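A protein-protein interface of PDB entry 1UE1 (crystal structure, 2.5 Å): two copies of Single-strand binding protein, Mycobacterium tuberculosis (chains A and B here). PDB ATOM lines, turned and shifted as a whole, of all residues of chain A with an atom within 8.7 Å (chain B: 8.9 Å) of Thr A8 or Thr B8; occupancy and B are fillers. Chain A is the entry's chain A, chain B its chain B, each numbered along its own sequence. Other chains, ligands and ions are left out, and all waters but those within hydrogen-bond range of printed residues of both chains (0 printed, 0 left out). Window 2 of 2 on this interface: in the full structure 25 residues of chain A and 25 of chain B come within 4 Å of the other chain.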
ATOM      1  N   THR A   5     -18.727  10.828   3.535  1.00  0.00           N
ATOM      2  CA  THR A   5     -17.819  11.446   4.474  1.00  0.00           C
ATOM      3  C   THR A   5     -18.285  11.047   5.877  1.00  0.00           C
ATOM      4  O   THR A   5     -19.411  11.343   6.284  1.00  0.00           O
ATOM      5  CB  THR A   5     -17.860  12.950   4.360  1.00  0.00           C
ATOM      6  OG1 THR A   5     -17.363  13.343   3.072  1.00  0.00           O
ATOM      7  CG2 THR A   5     -17.025  13.574   5.467  1.00  0.00           C
ATOM      8  N   THR A   6     -17.417  10.369   6.612  1.00  0.00           N
ATOM      9  CA  THR A   6     -17.767   9.929   7.943  1.00  0.00           C
ATOM     10  C   THR A   6     -16.970  10.658   9.001  1.00  0.00           C
ATOM     11  O   THR A   6     -15.919  11.233   8.719  1.00  0.00           O
ATOM     12  CB  THR A   6     -17.510   8.434   8.111  1.00  0.00           C
ATOM     13  OG1 THR A   6     -16.103   8.183   7.997  1.00  0.00           O
ATOM     14  CG2 THR A   6     -18.251   7.645   7.047  1.00  0.00           C
ATOM     15  N   ILE A   7     -17.487  10.628  10.226  1.00  0.00           N
ATOM     16  CA  ILE A   7     -16.827  11.262  11.348  1.00  0.00           C
ATOM     17  C   ILE A   7     -17.158  10.539  12.636  1.00  0.00           C
ATOM     18  O   ILE A   7     -18.090   9.738  12.701  1.00  0.00           O
ATOM     19  CB  ILE A   7     -17.266  12.713  11.532  1.00  0.00           C
ATOM     20  CG1 ILE A   7     -18.771  12.743  11.773  1.00  0.00           C
ATOM     21  CG2 ILE A   7     -16.820  13.573  10.335  1.00  0.00           C
ATOM     22  CD1 ILE A   7     -19.208  14.019  12.450  1.00  0.00           C
ATOM     23  N   THR A   8     -16.372  10.850  13.659  1.00  0.00           N
ATOM     24  CA  THR A   8     -16.521  10.303  14.994  1.00  0.00           C
ATOM     25  C   THR A   8     -16.585  11.499  15.909  1.00  0.00           C
ATOM     26  O   THR A   8     -15.685  12.329  15.908  1.00  0.00           O
ATOM     27  CB  THR A   8     -15.300   9.489  15.435  1.00  0.00           C
ATOM     28  OG1 THR A   8     -15.267   8.242  14.738  1.00  0.00           O
ATOM     29  CG2 THR A   8     -15.357   9.235  16.925  1.00  0.00           C
ATOM     30  N   ILE A   9     -17.649  11.608  16.680  1.00  0.00           N
ATOM     31  CA  ILE A   9     -17.731  12.720  17.596  1.00  0.00           C
ATOM     32  C   ILE A   9     -17.991  12.169  18.986  1.00  0.00           C
ATOM     33  O   ILE A   9     -18.862  11.314  19.174  1.00  0.00           O
ATOM     34  CB  ILE A   9     -18.837  13.744  17.184  1.00  0.00           C
ATOM     35  CG1 ILE A   9     -18.925  14.864  18.237  1.00  0.00           C
ATOM     36  CG2 ILE A   9     -20.175  13.048  17.016  1.00  0.00           C
ATOM     37  CD1 ILE A   9     -19.691  16.157  17.799  1.00  0.00           C
ATOM     38  N   VAL A  10     -17.177  12.623  19.936  1.00  0.00           N
ATOM     39  CA  VAL A  10     -17.297  12.239  21.331  1.00  0.00           C
ATOM     40  C   VAL A  10     -17.832  13.484  22.010  1.00  0.00           C
ATOM     41  O   VAL A  10     -17.292  14.559  21.828  1.00  0.00           O
ATOM     42  CB  VAL A  10     -15.932  11.876  21.942  1.00  0.00           C
ATOM     43  CG1 VAL A  10     -16.017  11.864  23.464  1.00  0.00           C
ATOM     44  CG2 VAL A  10     -15.496  10.514  21.445  1.00  0.00           C
ATOM     45  N   GLY A  11     -18.906  13.342  22.774  1.00  0.00           N
ATOM     46  CA  GLY A  11     -19.477  14.495  23.442  1.00  0.00           C
ATOM     47  C   GLY A  11     -20.654  14.015  24.254  1.00  0.00           C
ATOM     48  O   GLY A  11     -20.917  12.815  24.291  1.00  0.00           O
ATOM     49  N   VAL A  33     -25.405  15.818  19.870  1.00  0.00           N
ATOM     50  CA  VAL A  33     -24.223  15.594  20.682  1.00  0.00           C
ATOM     51  C   VAL A  33     -23.450  16.911  20.738  1.00  0.00           C
ATOM     52  O   VAL A  33     -23.266  17.584  19.718  1.00  0.00           O
ATOM     53  CB  VAL A  33     -23.341  14.502  20.060  1.00  0.00           C
ATOM     54  CG1 VAL A  33     -21.981  14.496  20.705  1.00  0.00           C
ATOM     55  CG2 VAL A  33     -24.008  13.157  20.220  1.00  0.00           C
ATOM     56  N   SER A  35     -19.913  18.314  21.631  1.00  0.00           N
ATOM     57  CA  SER A  35     -18.537  17.968  21.950  1.00  0.00           C
ATOM     58  C   SER A  35     -17.717  19.164  22.384  1.00  0.00           C
ATOM     59  O   SER A  35     -17.586  20.133  21.641  1.00  0.00           O
ATOM     60  CB  SER A  35     -17.878  17.312  20.745  1.00  0.00           C
ATOM     61  OG  SER A  35     -16.492  17.145  20.960  1.00  0.00           O
ATOM     62  N   LEU A  53     -18.642  21.959  19.742  1.00  0.00           N
ATOM     63  CA  LEU A  53     -19.262  21.487  18.508  1.00  0.00           C
ATOM     64  C   LEU A  53     -20.576  20.757  18.823  1.00  0.00           C
ATOM     65  O   LEU A  53     -20.603  19.796  19.595  1.00  0.00           O
ATOM     66  CB  LEU A  53     -18.321  20.526  17.783  1.00  0.00           C
ATOM     67  CG  LEU A  53     -18.539  20.374  16.281  1.00  0.00           C
ATOM     68  CD1 LEU A  53     -17.975  21.608  15.596  1.00  0.00           C
ATOM     69  CD2 LEU A  53     -17.845  19.128  15.771  1.00  0.00           C
ATOM     70  N   LEU A  55     -23.540  18.654  17.083  1.00  0.00           N
ATOM     71  CA  LEU A  55     -24.026  17.997  15.880  1.00  0.00           C
ATOM     72  C   LEU A  55     -25.337  17.222  16.037  1.00  0.00           C
ATOM     73  O   LEU A  55     -25.433  16.265  16.805  1.00  0.00           O
ATOM     74  CB  LEU A  55     -22.943  17.076  15.348  1.00  0.00           C
ATOM     75  CG  LEU A  55     -21.710  17.844  14.890  1.00  0.00           C
ATOM     76  CD1 LEU A  55     -20.674  16.878  14.355  1.00  0.00           C
ATOM     77  CD2 LEU A  55     -22.136  18.853  13.813  1.00  0.00           C
ATOM     78  N   VAL A  77     -21.088  10.176  24.827  1.00  0.00           N
ATOM     79  CA  VAL A  77     -21.189   9.156  23.807  1.00  0.00           C
ATOM     80  C   VAL A  77     -20.105   9.178  22.738  1.00  0.00           C
ATOM     81  O   VAL A  77     -19.360  10.152  22.584  1.00  0.00           O
ATOM     82  CB  VAL A  77     -22.542   9.269  23.081  1.00  0.00           C
ATOM     83  CG1 VAL A  77     -23.698   8.888  24.007  1.00  0.00           C
ATOM     84  CG2 VAL A  77     -22.727  10.692  22.596  1.00  0.00           C
ATOM     85  N   ILE A  78     -20.022   8.068  22.019  1.00  0.00           N
ATOM     86  CA  ILE A  78     -19.104   7.932  20.910  1.00  0.00           C
ATOM     87  C   ILE A  78     -20.067   7.709  19.762  1.00  0.00           C
ATOM     88  O   ILE A  78     -20.953   6.853  19.845  1.00  0.00           O
ATOM     89  CB  ILE A  78     -18.185   6.710  21.023  1.00  0.00           C
ATOM     90  CG1 ILE A  78     -17.413   6.752  22.337  1.00  0.00           C
ATOM     91  CG2 ILE A  78     -17.190   6.708  19.850  1.00  0.00           C
ATOM     92  CD1 ILE A  78     -16.520   5.566  22.531  1.00  0.00           C
ATOM     93  N   VAL A  79     -19.902   8.494  18.706  1.00  0.00           N
ATOM     94  CA  VAL A  79     -20.783   8.414  17.558  1.00  0.00           C
ATOM     95  C   VAL A  79     -20.030   8.386  16.241  1.00  0.00           C
ATOM     96  O   VAL A  79     -19.215   9.266  15.953  1.00  0.00           O
ATOM     97  CB  VAL A  79     -21.772   9.620  17.547  1.00  0.00           C
ATOM     98  CG1 VAL A  79     -22.529   9.669  16.244  1.00  0.00           C
ATOM     99  CG2 VAL A  79     -22.747   9.503  18.705  1.00  0.00           C
ATOM    100  N   SER A  80     -20.304   7.354  15.456  1.00  0.00           N
ATOM    101  CA  SER A  80     -19.701   7.206  14.143  1.00  0.00           C
ATOM    102  C   SER A  80     -20.862   7.246  13.162  1.00  0.00           C
ATOM    103  O   SER A  80     -21.817   6.471  13.277  1.00  0.00           O
ATOM    104  CB  SER A  80     -18.964   5.875  14.021  1.00  0.00           C
ATOM    105  OG  SER A  80     -18.407   5.716  12.726  1.00  0.00           O
ATOM    106  N   GLY A  81     -20.796   8.166  12.209  1.00  0.00           N
ATOM    107  CA  GLY A  81     -21.871   8.257  11.248  1.00  0.00           C
ATOM    108  C   GLY A  81     -21.437   8.945   9.983  1.00  0.00           C
ATOM    109  O   GLY A  81     -20.243   9.022   9.678  1.00  0.00           O
ATOM    110  N   ARG A  82     -22.411   9.465   9.254  1.00  0.00           N
ATOM    111  CA  ARG A  82     -22.136  10.126   7.998  1.00  0.00           C
ATOM    112  C   ARG A  82     -22.679  11.534   8.027  1.00  0.00           C
ATOM    113  O   ARG A  82     -23.822  11.751   8.423  1.00  0.00           O
ATOM    114  CB  ARG A  82     -22.786   9.333   6.860  1.00  0.00           C
ATOM    115  CG  ARG A  82     -22.272   7.897   6.754  1.00  0.00           C
ATOM    116  CD  ARG A  82     -22.992   7.056   5.693  1.00  0.00           C
ATOM    117  NE  ARG A  82     -24.174   6.367   6.211  1.00  0.00           N
ATOM    118  CZ  ARG A  82     -25.380   6.914   6.329  1.00  0.00           C
ATOM    119  NH1 ARG A  82     -25.578   8.171   5.958  1.00  0.00           N
ATOM    120  NH2 ARG A  82     -26.386   6.201   6.820  1.00  0.00           N
ATOM    121  N   LEU A  83     -21.851  12.492   7.623  1.00  0.00           N
ATOM    122  CA  LEU A  83     -22.278  13.882   7.578  1.00  0.00           C
ATOM    123  C   LEU A  83     -23.222  14.044   6.406  1.00  0.00           C
ATOM    124  O   LEU A  83     -22.958  13.552   5.310  1.00  0.00           O
ATOM    125  CB  LEU A  83     -21.100  14.815   7.354  1.00  0.00           C
ATOM    126  CG  LEU A  83     -20.209  15.160   8.530  1.00  0.00           C
ATOM    127  CD1 LEU A  83     -19.156  16.161   8.047  1.00  0.00           C
ATOM    128  CD2 LEU A  83     -21.040  15.749   9.655  1.00  0.00           C
ATOM    129  N   VAL A 101     -25.907  14.296  11.277  1.00  0.00           N
ATOM    130  CA  VAL A 101     -25.139  13.059  11.246  1.00  0.00           C
ATOM    131  C   VAL A 101     -26.025  11.814  11.263  1.00  0.00           C
ATOM    132  O   VAL A 101     -26.769  11.587  12.210  1.00  0.00           O
ATOM    133  CB  VAL A 101     -24.147  13.010  12.445  1.00  0.00           C
ATOM    134  CG1 VAL A 101     -23.546  11.613  12.596  1.00  0.00           C
ATOM    135  CG2 VAL A 101     -23.034  14.034  12.231  1.00  0.00           C
ATOM    136  N   GLU A 105     -23.109   3.860  14.279  1.00  0.00           N
ATOM    137  CA  GLU A 105     -22.926   3.233  15.582  1.00  0.00           C
ATOM    138  C   GLU A 105     -22.762   4.326  16.628  1.00  0.00           C
ATOM    139  O   GLU A 105     -22.192   5.393  16.365  1.00  0.00           O
ATOM    140  CB  GLU A 105     -21.685   2.339  15.609  1.00  0.00           C
ATOM    141  CG  GLU A 105     -21.632   1.227  14.582  1.00  0.00           C
ATOM    142  CD  GLU A 105     -22.344  -0.039  15.025  1.00  0.00           C
ATOM    143  OE1 GLU A 105     -22.275  -0.377  16.226  1.00  0.00           O
ATOM    144  OE2 GLU A 105     -22.954  -0.712  14.162  1.00  0.00           O
ATOM    145  N   ILE A 106     -23.265   4.032  17.817  1.00  0.00           N
ATOM    146  CA  ILE A 106     -23.217   4.935  18.950  1.00  0.00           C
ATOM    147  C   ILE A 106     -23.301   4.084  20.188  1.00  0.00           C
ATOM    148  O   ILE A 106     -23.968   3.044  20.192  1.00  0.00           O
ATOM    149  CB  ILE A 106     -24.424   5.875  18.986  1.00  0.00           C
ATOM    150  CG1 ILE A 106     -24.356   6.737  20.242  1.00  0.00           C
ATOM    151  CG2 ILE A 106     -25.710   5.062  18.994  1.00  0.00           C
ATOM    152  CD1 ILE A 106     -25.423   7.793  20.321  1.00  0.00           C
ATOM    153  N   THR B   5      -1.890   8.873  14.529  1.00  0.00           N
ATOM    154  CA  THR B   5      -2.806   8.382  13.515  1.00  0.00           C
ATOM    155  C   THR B   5      -3.960   7.784  14.305  1.00  0.00           C
ATOM    156  O   THR B   5      -3.750   6.935  15.164  1.00  0.00           O
ATOM    157  CB  THR B   5      -2.131   7.302  12.689  1.00  0.00           C
ATOM    158  OG1 THR B   5      -1.123   7.905  11.868  1.00  0.00           O
ATOM    159  CG2 THR B   5      -3.144   6.566  11.835  1.00  0.00           C
ATOM    160  N   THR B   6      -5.180   8.221  14.021  1.00  0.00           N
ATOM    161  CA  THR B   6      -6.327   7.735  14.769  1.00  0.00           C
ATOM    162  C   THR B   6      -7.334   6.908  13.980  1.00  0.00           C
ATOM    163  O   THR B   6      -7.465   7.053  12.764  1.00  0.00           O
ATOM    164  CB  THR B   6      -7.068   8.902  15.385  1.00  0.00           C
ATOM    165  OG1 THR B   6      -7.591   9.728  14.338  1.00  0.00           O
ATOM    166  CG2 THR B   6      -6.129   9.722  16.237  1.00  0.00           C
ATOM    167  N   ILE B   7      -8.052   6.043  14.691  1.00  0.00           N
ATOM    168  CA  ILE B   7      -9.053   5.202  14.067  1.00  0.00           C
ATOM    169  C   ILE B   7     -10.241   4.894  14.959  1.00  0.00           C
ATOM    170  O   ILE B   7     -10.132   4.835  16.188  1.00  0.00           O
ATOM    171  CB  ILE B   7      -8.481   3.836  13.611  1.00  0.00           C
ATOM    172  CG1 ILE B   7      -8.481   2.851  14.775  1.00  0.00           C
ATOM    173  CG2 ILE B   7      -7.070   4.007  13.062  1.00  0.00           C
ATOM    174  CD1 ILE B   7      -8.153   1.437  14.346  1.00  0.00           C
ATOM    175  N   THR B   8     -11.376   4.694  14.299  1.00  0.00           N
ATOM    176  CA  THR B   8     -12.625   4.344  14.940  1.00  0.00           C
ATOM    177  C   THR B   8     -12.945   2.961  14.395  1.00  0.00           C
ATOM    178  O   THR B   8     -13.245   2.819  13.214  1.00  0.00           O
ATOM    179  CB  THR B   8     -13.754   5.280  14.526  1.00  0.00           C
ATOM    180  OG1 THR B   8     -13.379   6.633  14.806  1.00  0.00           O
ATOM    181  CG2 THR B   8     -15.031   4.922  15.282  1.00  0.00           C
ATOM    182  N   ILE B   9     -12.860   1.948  15.246  1.00  0.00           N
ATOM    183  CA  ILE B   9     -13.139   0.581  14.843  1.00  0.00           C
ATOM    184  C   ILE B   9     -14.280  -0.005  15.649  1.00  0.00           C
ATOM    185  O   ILE B   9     -14.282   0.072  16.868  1.00  0.00           O
ATOM    186  CB  ILE B   9     -11.926  -0.323  15.053  1.00  0.00           C
ATOM    187  CG1 ILE B   9     -12.328  -1.786  14.885  1.00  0.00           C
ATOM    188  CG2 ILE B   9     -11.358  -0.113  16.432  1.00  0.00           C
ATOM    189  CD1 ILE B   9     -11.182  -2.753  15.099  1.00  0.00           C
ATOM    190  N   VAL B  10     -15.251  -0.584  14.950  1.00  0.00           N
ATOM    191  CA  VAL B  10     -16.389  -1.213  15.594  1.00  0.00           C
ATOM    192  C   VAL B  10     -16.208  -2.715  15.449  1.00  0.00           C
ATOM    193  O   VAL B  10     -15.735  -3.193  14.413  1.00  0.00           O
ATOM    194  CB  VAL B  10     -17.722  -0.799  14.947  1.00  0.00           C
ATOM    195  CG1 VAL B  10     -18.857  -1.516  15.645  1.00  0.00           C
ATOM    196  CG2 VAL B  10     -17.926   0.728  15.066  1.00  0.00           C
ATOM    197  N   GLY B  11     -16.566  -3.455  16.496  1.00  0.00           N
ATOM    198  CA  GLY B  11     -16.419  -4.897  16.462  1.00  0.00           C
ATOM    199  C   GLY B  11     -16.785  -5.536  17.780  1.00  0.00           C
ATOM    200  O   GLY B  11     -17.383  -4.887  18.643  1.00  0.00           O
ATOM    201  N   VAL B  33     -10.469  -6.272  19.319  1.00  0.00           N
ATOM    202  CA  VAL B  33     -11.751  -6.110  18.663  1.00  0.00           C
ATOM    203  C   VAL B  33     -11.778  -6.920  17.372  1.00  0.00           C
ATOM    204  O   VAL B  33     -10.839  -6.876  16.577  1.00  0.00           O
ATOM    205  CB  VAL B  33     -12.018  -4.627  18.328  1.00  0.00           C
ATOM    206  CG1 VAL B  33     -13.285  -4.506  17.510  1.00  0.00           C
ATOM    207  CG2 VAL B  33     -12.132  -3.807  19.612  1.00  0.00           C
ATOM    208  N   SER B  35     -13.524  -6.974  14.194  1.00  0.00           N
ATOM    209  CA  SER B  35     -14.330  -6.172  13.288  1.00  0.00           C
ATOM    210  C   SER B  35     -14.580  -6.978  12.026  1.00  0.00           C
ATOM    211  O   SER B  35     -13.642  -7.254  11.275  1.00  0.00           O
ATOM    212  CB  SER B  35     -13.574  -4.872  12.969  1.00  0.00           C
ATOM    213  OG  SER B  35     -14.120  -4.176  11.862  1.00  0.00           O
ATOM    214  N   LEU B  53     -11.090  -8.364  10.899  1.00  0.00           N
ATOM    215  CA  LEU B  53      -9.860  -7.700  11.317  1.00  0.00           C
ATOM    216  C   LEU B  53      -9.715  -7.848  12.838  1.00  0.00           C
ATOM    217  O   LEU B  53     -10.672  -7.642  13.582  1.00  0.00           O
ATOM    218  CB  LEU B  53      -9.929  -6.217  10.935  1.00  0.00           C
ATOM    219  CG  LEU B  53      -8.726  -5.318  11.239  1.00  0.00           C
ATOM    220  CD1 LEU B  53      -7.482  -5.852  10.554  1.00  0.00           C
ATOM    221  CD2 LEU B  53      -9.021  -3.910  10.766  1.00  0.00           C
ATOM    222  N   LEU B  55      -7.823  -6.442  16.098  1.00  0.00           N
ATOM    223  CA  LEU B  55      -6.971  -5.391  16.630  1.00  0.00           C
ATOM    224  C   LEU B  55      -6.899  -5.448  18.142  1.00  0.00           C
ATOM    225  O   LEU B  55      -7.928  -5.389  18.818  1.00  0.00           O
ATOM    226  CB  LEU B  55      -7.483  -4.022  16.190  1.00  0.00           C
ATOM    227  CG  LEU B  55      -7.132  -3.635  14.759  1.00  0.00           C
ATOM    228  CD1 LEU B  55      -7.916  -2.408  14.333  1.00  0.00           C
ATOM    229  CD2 LEU B  55      -5.646  -3.385  14.675  1.00  0.00           C
ATOM    230  N   VAL B  77     -18.560  -3.153  20.519  1.00  0.00           N
ATOM    231  CA  VAL B  77     -18.096  -1.890  21.053  1.00  0.00           C
ATOM    232  C   VAL B  77     -17.585  -0.912  19.997  1.00  0.00           C
ATOM    233  O   VAL B  77     -17.246  -1.291  18.872  1.00  0.00           O
ATOM    234  CB  VAL B  77     -16.985  -2.141  22.098  1.00  0.00           C
ATOM    235  CG1 VAL B  77     -17.530  -2.964  23.250  1.00  0.00           C
ATOM    236  CG2 VAL B  77     -15.818  -2.873  21.461  1.00  0.00           C
ATOM    237  N   ILE B  78     -17.555   0.360  20.367  1.00  0.00           N
ATOM    238  CA  ILE B  78     -17.054   1.397  19.481  1.00  0.00           C
ATOM    239  C   ILE B  78     -15.731   1.828  20.103  1.00  0.00           C
ATOM    240  O   ILE B  78     -15.662   2.110  21.300  1.00  0.00           O
ATOM    241  CB  ILE B  78     -18.019   2.612  19.412  1.00  0.00           C
ATOM    242  CG1 ILE B  78     -19.452   2.109  19.241  1.00  0.00           C
ATOM    243  CG2 ILE B  78     -17.632   3.533  18.228  1.00  0.00           C
ATOM    244  CD1 ILE B  78     -20.446   3.170  18.766  1.00  0.00           C
ATOM    245  N   VAL B  79     -14.674   1.865  19.305  1.00  0.00           N
ATOM    246  CA  VAL B  79     -13.378   2.256  19.836  1.00  0.00           C
ATOM    247  C   VAL B  79     -12.737   3.373  19.047  1.00  0.00           C
ATOM    248  O   VAL B  79     -12.522   3.255  17.840  1.00  0.00           O
ATOM    249  CB  VAL B  79     -12.394   1.053  19.857  1.00  0.00           C
ATOM    250  CG1 VAL B  79     -10.981   1.523  20.175  1.00  0.00           C
ATOM    251  CG2 VAL B  79     -12.852   0.020  20.881  1.00  0.00           C
ATOM    252  N   SER B  80     -12.446   4.467  19.734  1.00  0.00           N
ATOM    253  CA  SER B  80     -11.763   5.588  19.108  1.00  0.00           C
ATOM    254  C   SER B  80     -10.374   5.549  19.736  1.00  0.00           C
ATOM    255  O   SER B  80     -10.253   5.548  20.953  1.00  0.00           O
ATOM    256  CB  SER B  80     -12.458   6.908  19.447  1.00  0.00           C
ATOM    257  OG  SER B  80     -11.880   7.990  18.737  1.00  0.00           O
ATOM    258  N   GLY B  81      -9.326   5.493  18.925  1.00  0.00           N
ATOM    259  CA  GLY B  81      -7.997   5.434  19.498  1.00  0.00           C
ATOM    260  C   GLY B  81      -6.860   5.814  18.570  1.00  0.00           C
ATOM    261  O   GLY B  81      -7.078   6.309  17.468  1.00  0.00           O
ATOM    262  N   ARG B  82      -5.638   5.577  19.028  1.00  0.00           N
ATOM    263  CA  ARG B  82      -4.448   5.908  18.260  1.00  0.00           C
ATOM    264  C   ARG B  82      -3.618   4.672  17.997  1.00  0.00           C
ATOM    265  O   ARG B  82      -3.375   3.869  18.898  1.00  0.00           O
ATOM    266  CB  ARG B  82      -3.610   6.945  19.019  1.00  0.00           C
ATOM    267  CG  ARG B  82      -4.297   8.298  19.155  1.00  0.00           C
ATOM    268  CD  ARG B  82      -3.678   9.165  20.232  1.00  0.00           C
ATOM    269  NE  ARG B  82      -4.014   8.730  21.594  1.00  0.00           N
ATOM    270  CZ  ARG B  82      -3.231   7.983  22.372  1.00  0.00           C
ATOM    271  NH1 ARG B  82      -2.047   7.566  21.945  1.00  0.00           N
ATOM    272  NH2 ARG B  82      -3.628   7.661  23.593  1.00  0.00           N
ATOM    273  N   LEU B  83      -3.188   4.523  16.749  1.00  0.00           N
ATOM    274  CA  LEU B  83      -2.378   3.389  16.357  1.00  0.00           C
ATOM    275  C   LEU B  83      -0.976   3.552  16.910  1.00  0.00           C
ATOM    276  O   LEU B  83      -0.366   4.616  16.797  1.00  0.00           O
ATOM    277  CB  LEU B  83      -2.320   3.268  14.832  1.00  0.00           C
ATOM    278  CG  LEU B  83      -3.648   2.994  14.132  1.00  0.00           C
ATOM    279  CD1 LEU B  83      -3.389   2.718  12.652  1.00  0.00           C
ATOM    280  CD2 LEU B  83      -4.352   1.801  14.799  1.00  0.00           C
ATOM    281  N   VAL B 101      -3.885  -0.804  19.132  1.00  0.00           N
ATOM    282  CA  VAL B 101      -4.589   0.440  19.398  1.00  0.00           C
ATOM    283  C   VAL B 101      -4.531   0.872  20.855  1.00  0.00           C
ATOM    284  O   VAL B 101      -4.641   0.050  21.763  1.00  0.00           O
ATOM    285  CB  VAL B 101      -6.081   0.320  18.982  1.00  0.00           C
ATOM    286  CG1 VAL B 101      -6.835   1.584  19.333  1.00  0.00           C
ATOM    287  CG2 VAL B 101      -6.179   0.058  17.507  1.00  0.00           C
ATOM    288  N   GLU B 105     -11.303   6.448  23.911  1.00  0.00           N
ATOM    289  CA  GLU B 105     -12.707   6.387  24.261  1.00  0.00           C
ATOM    290  C   GLU B 105     -13.223   5.081  23.695  1.00  0.00           C
ATOM    291  O   GLU B 105     -12.861   4.681  22.584  1.00  0.00           O
ATOM    292  CB  GLU B 105     -13.473   7.559  23.647  1.00  0.00           C
ATOM    293  CG  GLU B 105     -12.932   8.908  24.038  1.00  0.00           C
ATOM    294  CD  GLU B 105     -13.777   9.588  25.065  1.00  0.00           C
ATOM    295  OE1 GLU B 105     -14.449   8.884  25.842  1.00  0.00           O
ATOM    296  OE2 GLU B 105     -13.765  10.834  25.102  1.00  0.00           O
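OG1 of Thr B8 lies within hydrogen-bond range of OG1 of Thr A8.
O of Val B10 lies close to OG of Ser B35. The backbone carbonyl oxygen (O) of Val A10 lies within hydrogen-bond range of the side-chain hydroxyl (OG) of Ser A35, at 2.8 Å. N of Ser A80 sits at hydrogen-bond distance from O of Glu A105 (2.9 Å). The backbone NH of Ser B80 is in hydrogen-bond range of the backbone carbonyl oxygen of Glu B105 (2.9 Å).
Val A10 touches Glu B105 (CG1 to OE2, 3.0 Å). CG2 of Ile B78 touches CG2 of Ile A78 (3.6 Å). Glu B105 touches Ile A78 (C to CD1, 3.5 Å). Glu A105 touches Val B10 (OE1 to CG1, 3.6 Å). Glu A105 touches Ile B78 (C to CD1, 3.4 Å). CD1 of Ile B78 touches N of Ile A106, at 3.1 Å.
Thr A8 touches one residue of chain B. Of chain A, only Thr A8 comes within 4 Å of Thr B8. Ile A7 touches none of the printed residues of chain B. No residue of chain A comes within 4 Å of Ile B7. Of the printed residues of chain B, Ile A78 touches Ile B78 (3.6 Å) and Glu B105 (3.5 Å). Of the printed residues of chain B, Glu A105 touches Val B10 (3.6 Å) and Ile B78 (3.4 Å). Of the printed residues of chain A, Val B10 touches Glu A105. Thr A6 touches none of the printed residues of chain B. Val B101 touches none of the printed residues of chain A.
Of the 21 printed residues of chain A, 5 touch a printed residue of chain B. Along chain A the printed residues that touch a printed residue of chain B span positions 8 to 106. Of the 20 printed residues of chain B, 4 touch a printed residue of chain A. Printed residues of chain B that touch a printed residue of chain A: Thr B8, Val B10, Ile B78 and Glu B105. Hydrophobic or aromatic side chains of chain B that line the printed part of chain A: Val B10 and Ile B78. Among the printed residues, 7 pairs touch across the chains. Among the printed residues, no Asp or Glu carboxylate lies within 4 Å of a Lys or Arg side-chain nitrogen of the other chain.
Thr B8 touches its own counterpart, Thr A8. Val A10 touches Glu B105, and with the chains exchanged Glu A105 touches Val B10. Ile A78 touches its own counterpart, Ile B78. Ile A78 touches Glu B105, and with the chains exchanged Glu A105 touches Ile B78.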
